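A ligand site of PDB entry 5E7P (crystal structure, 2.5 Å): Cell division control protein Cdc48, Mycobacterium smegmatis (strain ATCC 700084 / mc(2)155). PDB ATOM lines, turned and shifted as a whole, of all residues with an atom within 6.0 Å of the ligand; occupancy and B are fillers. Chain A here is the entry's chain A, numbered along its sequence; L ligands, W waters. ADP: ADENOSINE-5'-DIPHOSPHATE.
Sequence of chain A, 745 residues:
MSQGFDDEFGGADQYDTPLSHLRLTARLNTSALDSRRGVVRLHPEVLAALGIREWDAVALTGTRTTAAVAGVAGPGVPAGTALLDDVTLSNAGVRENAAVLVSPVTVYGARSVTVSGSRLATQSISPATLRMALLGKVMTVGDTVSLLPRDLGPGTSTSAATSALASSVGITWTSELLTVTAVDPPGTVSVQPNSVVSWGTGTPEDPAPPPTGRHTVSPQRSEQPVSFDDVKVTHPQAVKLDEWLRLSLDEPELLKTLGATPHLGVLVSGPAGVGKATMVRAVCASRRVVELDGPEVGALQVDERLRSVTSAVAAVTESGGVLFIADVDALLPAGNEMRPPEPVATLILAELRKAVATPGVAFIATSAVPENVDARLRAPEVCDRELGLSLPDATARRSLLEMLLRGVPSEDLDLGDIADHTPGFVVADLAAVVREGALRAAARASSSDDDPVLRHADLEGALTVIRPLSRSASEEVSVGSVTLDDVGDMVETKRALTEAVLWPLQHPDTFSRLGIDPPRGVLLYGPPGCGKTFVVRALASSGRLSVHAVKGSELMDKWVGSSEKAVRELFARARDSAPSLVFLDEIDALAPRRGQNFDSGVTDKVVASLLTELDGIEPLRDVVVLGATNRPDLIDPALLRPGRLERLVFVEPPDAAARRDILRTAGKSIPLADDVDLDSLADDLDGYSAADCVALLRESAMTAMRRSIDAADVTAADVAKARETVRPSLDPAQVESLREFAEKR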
ATOM      1  N   MET A 132      20.780   6.227  -5.754  1.00  0.00           N
ATOM      2  CA  MET A 132      20.670   5.857  -7.159  1.00  0.00           C
ATOM      3  C   MET A 132      20.008   6.971  -7.975  1.00  0.00           C
ATOM      4  O   MET A 132      20.452   7.309  -9.075  1.00  0.00           O
ATOM      5  CB  MET A 132      19.877   4.564  -7.311  1.00  0.00           C
ATOM      6  CG  MET A 132      19.691   4.104  -8.744  1.00  0.00           C
ATOM      7  SD  MET A 132      18.585   2.689  -8.879  1.00  0.00           S
ATOM      8  CE  MET A 132      19.403   1.530  -7.785  1.00  0.00           C
ATOM      9  N   LEU A 135      22.327  10.180  -8.055  1.00  0.00           N
ATOM     10  CA  LEU A 135      23.730   9.905  -8.339  1.00  0.00           C
ATOM     11  C   LEU A 135      24.333  10.952  -9.287  1.00  0.00           C
ATOM     12  O   LEU A 135      23.813  11.192 -10.370  1.00  0.00           O
ATOM     13  CB  LEU A 135      23.889   8.505  -8.932  1.00  0.00           C
ATOM     14  CG  LEU A 135      25.305   7.917  -8.969  1.00  0.00           C
ATOM     15  CD1 LEU A 135      25.862   7.788  -7.553  1.00  0.00           C
ATOM     16  CD2 LEU A 135      25.302   6.566  -9.668  1.00  0.00           C
ATOM     17  N   PRO A 193      28.797   7.031  -5.442  1.00  0.00           N
ATOM     18  CA  PRO A 193      28.457   5.674  -4.972  1.00  0.00           C
ATOM     19  C   PRO A 193      28.900   5.414  -3.534  1.00  0.00           C
ATOM     20  O   PRO A 193      28.260   4.628  -2.835  1.00  0.00           O
ATOM     21  CB  PRO A 193      29.227   4.776  -5.931  1.00  0.00           C
ATOM     22  CG  PRO A 193      29.337   5.574  -7.188  1.00  0.00           C
ATOM     23  CD  PRO A 193      29.497   6.998  -6.746  1.00  0.00           C
ATOM     24  N   PRO A 225      19.799  -9.723 -10.256  1.00  0.00           N
ATOM     25  CA  PRO A 225      19.411  -8.801 -11.338  1.00  0.00           C
ATOM     26  C   PRO A 225      20.373  -8.888 -12.522  1.00  0.00           C
ATOM     27  O   PRO A 225      19.932  -8.816 -13.677  1.00  0.00           O
ATOM     28  CB  PRO A 225      19.509  -7.419 -10.673  1.00  0.00           C
ATOM     29  CG  PRO A 225      20.442  -7.610  -9.522  1.00  0.00           C
ATOM     30  CD  PRO A 225      20.178  -9.002  -9.038  1.00  0.00           C
ATOM     31  N   VAL A 226      21.665  -9.043 -12.250  1.00  0.00           N
ATOM     32  CA  VAL A 226      22.670  -9.154 -13.295  1.00  0.00           C
ATOM     33  C   VAL A 226      23.474 -10.441 -13.154  1.00  0.00           C
ATOM     34  O   VAL A 226      24.085 -10.685 -12.112  1.00  0.00           O
ATOM     35  CB  VAL A 226      23.632  -7.942 -13.271  1.00  0.00           C
ATOM     36  CG1 VAL A 226      24.567  -7.996 -14.458  1.00  0.00           C
ATOM     37  CG2 VAL A 226      22.844  -6.645 -13.276  1.00  0.00           C
ATOM     38  N   ASP A 230      26.652 -11.912 -17.938  1.00  0.00           N
ATOM     39  CA  ASP A 230      26.440 -10.518 -18.327  1.00  0.00           C
ATOM     40  C   ASP A 230      27.607  -9.635 -17.887  1.00  0.00           C
ATOM     41  O   ASP A 230      27.999  -8.706 -18.592  1.00  0.00           O
ATOM     42  CB  ASP A 230      25.149  -9.984 -17.727  1.00  0.00           C
ATOM     43  CG  ASP A 230      23.911 -10.442 -18.471  1.00  0.00           C
ATOM     44  OD1 ASP A 230      23.965 -10.495 -19.725  1.00  0.00           O
ATOM     45  OD2 ASP A 230      22.893 -10.750 -17.817  1.00  0.00           O
ATOM     46  N   GLY A 270      38.284   0.648  -9.354  1.00  0.00           N
ATOM     47  CA  GLY A 270      37.903   1.092 -10.672  1.00  0.00           C
ATOM     48  C   GLY A 270      36.950   2.267 -10.594  1.00  0.00           C
ATOM     49  O   GLY A 270      36.422   2.559  -9.515  1.00  0.00           O
ATOM     50  N   PRO A 271      36.702   2.934 -11.733  1.00  0.00           N
ATOM     51  CA  PRO A 271      35.890   4.158 -11.815  1.00  0.00           C
ATOM     52  C   PRO A 271      34.537   4.050 -11.103  1.00  0.00           C
ATOM     53  O   PRO A 271      33.964   2.967 -11.006  1.00  0.00           O
ATOM     54  CB  PRO A 271      35.681   4.310 -13.326  1.00  0.00           C
ATOM     55  CG  PRO A 271      36.861   3.655 -13.931  1.00  0.00           C
ATOM     56  CD  PRO A 271      37.155   2.483 -13.060  1.00  0.00           C
ATOM     57  N   ALA A 272      34.046   5.181 -10.617  1.00  0.00           N
ATOM     58  CA  ALA A 272      32.775   5.208  -9.896  1.00  0.00           C
ATOM     59  C   ALA A 272      31.619   4.802 -10.812  1.00  0.00           C
ATOM     60  O   ALA A 272      31.468   5.348 -11.902  1.00  0.00           O
ATOM     61  CB  ALA A 272      32.534   6.597  -9.299  1.00  0.00           C
ATOM     62  N   GLY A 273      30.812   3.847 -10.357  1.00  0.00           N
ATOM     63  CA  GLY A 273      29.657   3.410 -11.110  1.00  0.00           C
ATOM     64  C   GLY A 273      29.998   2.548 -12.301  1.00  0.00           C
ATOM     65  O   GLY A 273      29.156   2.314 -13.168  1.00  0.00           O
ATOM     66  N   VAL A 274      31.232   2.063 -12.348  1.00  0.00           N
ATOM     67  CA  VAL A 274      31.660   1.209 -13.445  1.00  0.00           C
ATOM     68  C   VAL A 274      31.030  -0.177 -13.331  1.00  0.00           C
ATOM     69  O   VAL A 274      30.913  -0.897 -14.322  1.00  0.00           O
ATOM     70  CB  VAL A 274      33.191   1.097 -13.537  1.00  0.00           C
ATOM     71  CG1 VAL A 274      33.716   0.105 -12.512  1.00  0.00           C
ATOM     72  CG2 VAL A 274      33.622   0.703 -14.942  1.00  0.00           C
ATOM     73  N   GLY A 275      30.609  -0.539 -12.124  1.00  0.00           N
ATOM     74  CA  GLY A 275      29.934  -1.808 -11.897  1.00  0.00           C
ATOM     75  C   GLY A 275      30.709  -2.762 -11.006  1.00  0.00           C
ATOM     76  O   GLY A 275      30.637  -3.980 -11.187  1.00  0.00           O
ATOM     77  N   LYS A 276      31.433  -2.219 -10.027  1.00  0.00           N
ATOM     78  CA  LYS A 276      32.238  -3.051  -9.122  1.00  0.00           C
ATOM     79  C   LYS A 276      31.382  -3.908  -8.199  1.00  0.00           C
ATOM     80  O   LYS A 276      31.630  -5.107  -8.042  1.00  0.00           O
ATOM     81  CB  LYS A 276      33.199  -2.179  -8.311  1.00  0.00           C
ATOM     82  CG  LYS A 276      34.194  -1.413  -9.153  1.00  0.00           C
ATOM     83  CD  LYS A 276      35.108  -0.582  -8.271  1.00  0.00           C
ATOM     84  CE  LYS A 276      34.336   0.455  -7.477  1.00  0.00           C
ATOM     85  NZ  LYS A 276      33.708   1.469  -8.370  1.00  0.00           N
ATOM     86  N   ALA A 277      30.377  -3.306  -7.573  1.00  0.00           N
ATOM     87  CA  ALA A 277      29.523  -4.011  -6.626  1.00  0.00           C
ATOM     88  C   ALA A 277      28.646  -5.038  -7.341  1.00  0.00           C
ATOM     89  O   ALA A 277      28.428  -6.133  -6.838  1.00  0.00           O
ATOM     90  CB  ALA A 277      28.675  -3.036  -5.817  1.00  0.00           C
ATOM     91  N   THR A 278      28.142  -4.658  -8.503  1.00  0.00           N
ATOM     92  CA  THR A 278      27.319  -5.556  -9.315  1.00  0.00           C
ATOM     93  C   THR A 278      28.099  -6.788  -9.737  1.00  0.00           C
ATOM     94  O   THR A 278      27.578  -7.903  -9.756  1.00  0.00           O
ATOM     95  CB  THR A 278      26.759  -4.832 -10.553  1.00  0.00           C
ATOM     96  OG1 THR A 278      25.894  -3.754 -10.133  1.00  0.00           O
ATOM     97  CG2 THR A 278      25.964  -5.781 -11.430  1.00  0.00           C
ATOM     98  N   MET A 279      29.376  -6.598 -10.083  1.00  0.00           N
ATOM     99  CA  MET A 279      30.235  -7.710 -10.457  1.00  0.00           C
ATOM    100  C   MET A 279      30.405  -8.687  -9.299  1.00  0.00           C
ATOM    101  O   MET A 279      30.364  -9.902  -9.492  1.00  0.00           O
ATOM    102  CB  MET A 279      31.614  -7.201 -10.901  1.00  0.00           C
ATOM    103  CG  MET A 279      32.599  -8.340 -11.199  1.00  0.00           C
ATOM    104  SD  MET A 279      34.279  -7.803 -11.578  1.00  0.00           S
ATOM    105  CE  MET A 279      34.870  -7.348  -9.947  1.00  0.00           C
ATOM    106  N   ARG A 281      28.406  -9.215  -6.653  1.00  0.00           N
ATOM    107  CA  ARG A 281      27.158  -9.931  -6.416  1.00  0.00           C
ATOM    108  C   ARG A 281      26.930 -11.020  -7.461  1.00  0.00           C
ATOM    109  O   ARG A 281      26.467 -12.121  -7.140  1.00  0.00           O
ATOM    110  CB  ARG A 281      25.977  -8.958  -6.385  1.00  0.00           C
ATOM    111  CG  ARG A 281      26.150  -7.829  -5.389  1.00  0.00           C
ATOM    112  CD  ARG A 281      24.869  -7.025  -5.214  1.00  0.00           C
ATOM    113  NE  ARG A 281      25.075  -5.902  -4.302  1.00  0.00           N
ATOM    114  CZ  ARG A 281      25.322  -4.651  -4.685  1.00  0.00           C
ATOM    115  NH1 ARG A 281      25.398  -4.362  -5.971  1.00  0.00           N
ATOM    116  NH2 ARG A 281      25.503  -3.701  -3.777  1.00  0.00           N
ATOM    117  N   ASP A 327      31.968  -0.294  -1.228  1.00  0.00           N
ATOM    118  CA  ASP A 327      32.529   1.033  -0.972  1.00  0.00           C
ATOM    119  C   ASP A 327      33.049   1.172   0.453  1.00  0.00           C
ATOM    120  O   ASP A 327      32.536   1.966   1.250  1.00  0.00           O
ATOM    121  CB  ASP A 327      31.515   2.125  -1.325  1.00  0.00           C
ATOM    122  CG  ASP A 327      31.018   2.011  -2.761  1.00  0.00           C
ATOM    123  OD1 ASP A 327      31.761   2.400  -3.686  1.00  0.00           O
ATOM    124  OD2 ASP A 327      29.886   1.517  -2.960  1.00  0.00           O
ATOM    125  N   THR A 366      34.809  -3.294  -2.121  1.00  0.00           N
ATOM    126  CA  THR A 366      34.972  -2.411  -3.261  1.00  0.00           C
ATOM    127  C   THR A 366      35.333  -0.999  -2.824  1.00  0.00           C
ATOM    128  O   THR A 366      35.093  -0.602  -1.680  1.00  0.00           O
ATOM    129  CB  THR A 366      33.705  -2.352  -4.131  1.00  0.00           C
ATOM    130  OG1 THR A 366      32.611  -1.881  -3.343  1.00  0.00           O
ATOM    131  CG2 THR A 366      33.372  -3.734  -4.699  1.00  0.00           C
ATOM    132  N   LEU A 389      39.089  -2.590 -12.195  1.00  0.00           N
ATOM    133  CA  LEU A 389      38.168  -2.599 -13.328  1.00  0.00           C
ATOM    134  C   LEU A 389      38.439  -1.426 -14.263  1.00  0.00           C
ATOM    135  O   LEU A 389      39.095  -0.453 -13.894  1.00  0.00           O
ATOM    136  CB  LEU A 389      36.715  -2.577 -12.854  1.00  0.00           C
ATOM    137  CG  LEU A 389      36.024  -3.946 -12.715  1.00  0.00           C
ATOM    138  CD1 LEU A 389      36.892  -4.910 -11.928  1.00  0.00           C
ATOM    139  CD2 LEU A 389      34.656  -3.797 -12.065  1.00  0.00           C
ATOM    140  N   LEU A 400      26.438  -2.724 -23.126  1.00  0.00           N
ATOM    141  CA  LEU A 400      25.736  -2.309 -21.925  1.00  0.00           C
ATOM    142  C   LEU A 400      24.353  -1.733 -22.251  1.00  0.00           C
ATOM    143  O   LEU A 400      23.374  -2.043 -21.563  1.00  0.00           O
ATOM    144  CB  LEU A 400      26.569  -1.306 -21.146  1.00  0.00           C
ATOM    145  CG  LEU A 400      27.851  -1.866 -20.514  1.00  0.00           C
ATOM    146  CD1 LEU A 400      28.702  -0.747 -19.923  1.00  0.00           C
ATOM    147  CD2 LEU A 400      27.506  -2.907 -19.460  1.00  0.00           C
ATOM    148  N   MET A 403      21.911  -4.371 -23.140  1.00  0.00           N
ATOM    149  CA  MET A 403      21.563  -5.026 -21.888  1.00  0.00           C
ATOM    150  C   MET A 403      20.550  -4.208 -21.080  1.00  0.00           C
ATOM    151  O   MET A 403      19.587  -4.742 -20.538  1.00  0.00           O
ATOM    152  CB  MET A 403      22.815  -5.274 -21.060  1.00  0.00           C
ATOM    153  CG  MET A 403      22.567  -6.035 -19.775  1.00  0.00           C
ATOM    154  SD  MET A 403      24.093  -6.311 -18.837  1.00  0.00           S
ATOM    155  CE  MET A 403      25.139  -7.062 -20.083  1.00  0.00           C
ATOM    156  N   LEU A 404      20.786  -2.896 -21.024  1.00  0.00           N
ATOM    157  CA  LEU A 404      19.904  -1.989 -20.284  1.00  0.00           C
ATOM    158  C   LEU A 404      18.536  -1.843 -20.941  1.00  0.00           C
ATOM    159  O   LEU A 404      17.576  -1.395 -20.306  1.00  0.00           O
ATOM    160  CB  LEU A 404      20.555  -0.602 -20.150  1.00  0.00           C
ATOM    161  CG  LEU A 404      21.754  -0.490 -19.199  1.00  0.00           C
ATOM    162  CD1 LEU A 404      22.540   0.773 -19.467  1.00  0.00           C
ATOM    163  CD2 LEU A 404      21.273  -0.531 -17.756  1.00  0.00           C
ATOM    164  N   VAL A 427      28.429   2.373 -16.837  1.00  0.00           N
ATOM    165  CA  VAL A 427      27.102   1.768 -16.905  1.00  0.00           C
ATOM    166  C   VAL A 427      26.067   2.566 -16.099  1.00  0.00           C
ATOM    167  O   VAL A 427      24.906   2.665 -16.499  1.00  0.00           O
ATOM    168  CB  VAL A 427      27.122   0.274 -16.464  1.00  0.00           C
ATOM    169  CG1 VAL A 427      27.657   0.128 -15.041  1.00  0.00           C
ATOM    170  CG2 VAL A 427      25.735  -0.348 -16.590  1.00  0.00           C
ATOM    171  N   ALA A 428      26.507   3.140 -14.983  1.00  0.00           N
ATOM    172  CA  ALA A 428      25.643   3.956 -14.142  1.00  0.00           C
ATOM    173  C   ALA A 428      25.097   5.141 -14.942  1.00  0.00           C
ATOM    174  O   ALA A 428      23.906   5.442 -14.885  1.00  0.00           O
ATOM    175  CB  ALA A 428      26.392   4.437 -12.911  1.00  0.00           C
ATOM    176  N   ALA A 431      22.783   3.909 -17.717  1.00  0.00           N
ATOM    177  CA  ALA A 431      21.496   3.593 -17.124  1.00  0.00           C
ATOM    178  C   ALA A 431      20.678   4.864 -16.935  1.00  0.00           C
ATOM    179  O   ALA A 431      19.487   4.892 -17.251  1.00  0.00           O
ATOM    180  CB  ALA A 431      21.692   2.880 -15.794  1.00  0.00           C
HETATM  181  PB  ADP L   1      30.314   0.625  -8.570  1.00  0.00           P
HETATM  182  O1B ADP L   1      30.354   2.058  -8.110  1.00  0.00           O
HETATM  183  O2B ADP L   1      30.072  -0.379  -7.478  1.00  0.00           O
HETATM  184  O3B ADP L   1      31.432   0.240  -9.513  1.00  0.00           O
HETATM  185  PA  ADP L   1      27.782  -0.445  -9.207  1.00  0.00           P
HETATM  186  O1A ADP L   1      27.014   0.034  -7.999  1.00  0.00           O
HETATM  187  O2A ADP L   1      28.330  -1.851  -9.212  1.00  0.00           O
HETATM  188  O3A ADP L   1      28.971   0.610  -9.454  1.00  0.00           O
HETATM  189  O5' ADP L   1      26.848  -0.208 -10.484  1.00  0.00           O
HETATM  190  C5' ADP L   1      26.673   1.120 -10.943  1.00  0.00           C
HETATM  191  C4' ADP L   1      25.181   1.307 -11.163  1.00  0.00           C
HETATM  192  O4' ADP L   1      24.820   0.769 -12.435  1.00  0.00           O
HETATM  193  C3' ADP L   1      24.390   0.565 -10.103  1.00  0.00           C
HETATM  194  O3' ADP L   1      23.441   1.451  -9.485  1.00  0.00           O
HETATM  195  C2' ADP L   1      23.656  -0.545 -10.827  1.00  0.00           C
HETATM  196  O2' ADP L   1      22.283  -0.565 -10.433  1.00  0.00           O
HETATM  197  C1' ADP L   1      23.784  -0.196 -12.300  1.00  0.00           C
HETATM  198  N9  ADP L   1      24.142  -1.385 -13.119  1.00  0.00           N
HETATM  199  C8  ADP L   1      25.348  -1.967 -13.170  1.00  0.00           C
HETATM  200  N7  ADP L   1      25.336  -3.022 -14.023  1.00  0.00           N
HETATM  201  C5  ADP L   1      24.092  -3.113 -14.539  1.00  0.00           C
HETATM  202  C6  ADP L   1      23.387  -3.997 -15.497  1.00  0.00           C
HETATM  203  N6  ADP L   1      24.032  -5.029 -16.099  1.00  0.00           N
HETATM  204  N1  ADP L   1      22.082  -3.757 -15.749  1.00  0.00           N
HETATM  205  C2  ADP L   1      21.427  -2.737 -15.153  1.00  0.00           C
HETATM  206  N3  ADP L   1      22.011  -1.896 -14.276  1.00  0.00           N
HETATM  207  C4  ADP L   1      23.311  -2.034 -13.935  1.00  0.00           C
HETATM  208  O   HOH W   1      25.332  -1.909  -6.654  1.00  0.00           O
HETATM  209  O   HOH W   2      28.679   0.677  -5.395  1.00  0.00           O
HETATM  210  O   HOH W   3      31.712  -0.068  -5.267  1.00  0.00           O
HETATM  211  O   HOH W   4      27.662   2.539  -8.053  1.00  0.00           O
HETATM  212  O   HOH W   5      32.069   3.416  -6.956  1.00  0.00           O
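The side-chain amino group (NZ) of Lys 276 sits at hydrogen-bond distance from the backbone carbonyl oxygen (O) of Pro 271 (3.0 Å). O of Gly 270 is in hydrogen-bond range of NZ of Lys 276 (3.1 Å). The backbone carbonyl oxygen (O) of Gly 273 sits at hydrogen-bond distance from the backbone NH (N) of Ala 428 (3.3 Å).
CB of Pro 193 touches O1B of the ligand, 3.7 Å away. Val 226 touches the ligand (CG1 to N6, 3.4 Å). Leu 404 touches the ligand. Val 427 touches the ligand (CG1 to C8, 3.6 Å). CA of Ala 428 touches O4' of the ligand, at 3.7 Å. Hydrophobic or aromatic side chains that line the ligand: Pro 193, Val 226, Val 274, Ala 277, Met 403, Leu 404, Val 427 and Ala 428. Within 4 Å of the ligand: Pro 193, Val 226, Gly 273, Val 274, Gly 275, Lys 276, Ala 277, Thr 278, Met 403, Leu 404, Val 427 and Ala 428. The nearest printed residue that does not touch the ligand is Pro 271 (4.01 Å).
Water W5 lies within hydrogen-bond range of O1B of the ligand (2.5 Å), NZ of Lys 276 (2.9 Å) and OD1 of Asp 327 (3.4 Å). Water W2 lies within hydrogen-bond range of an oxygen (O2B) of the ligand (2.7 Å) and the side-chain carboxylate of Asp 327 (2.8 Å). Water W3 lies within hydrogen-bond range of an oxygen (O2B) of the ligand (2.8 Å), the side-chain hydroxyl (OG1) of Thr 366 (2.8 Å) and the side-chain carboxylate (OD1) of Asp 327 (2.9 Å). Water W1 bridges NH1 of Arg 281 (2.5 Å) and O1A of the ligand (2.9 Å).
The backbone NH of Lys 276 is in hydrogen-bond range of an oxygen (O3B) of the ligand (2.5 Å). The side-chain amino group of Lys 276 lies within salt-bridge range of an oxygen (O3B) of the ligand (2.8 Å). An oxygen (O3B) of the ligand lies within hydrogen-bond range of the backbone NH of Gly 275. The backbone NH of Thr 278 is in hydrogen-bond range of an oxygen (O2A) of the ligand. The side-chain hydroxyl (OG1) of Thr 278 sits at hydrogen-bond distance from an oxygen (O2A) of the ligand (3.2 Å). N of Gly 273 is in hydrogen-bond range of O1B of the ligand (2.9 Å). The backbone NH (N) of Ala 277 sits at hydrogen-bond distance from an oxygen (O2B) of the ligand (2.9 Å). The side-chain sulfur of Met 403 sits at hydrogen-bond distance from a nitrogen (N6) of the ligand (3.0 Å). The backbone NH of Val 274 is in hydrogen-bond range of an oxygen (O3B) of the ligand (3.4 Å).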
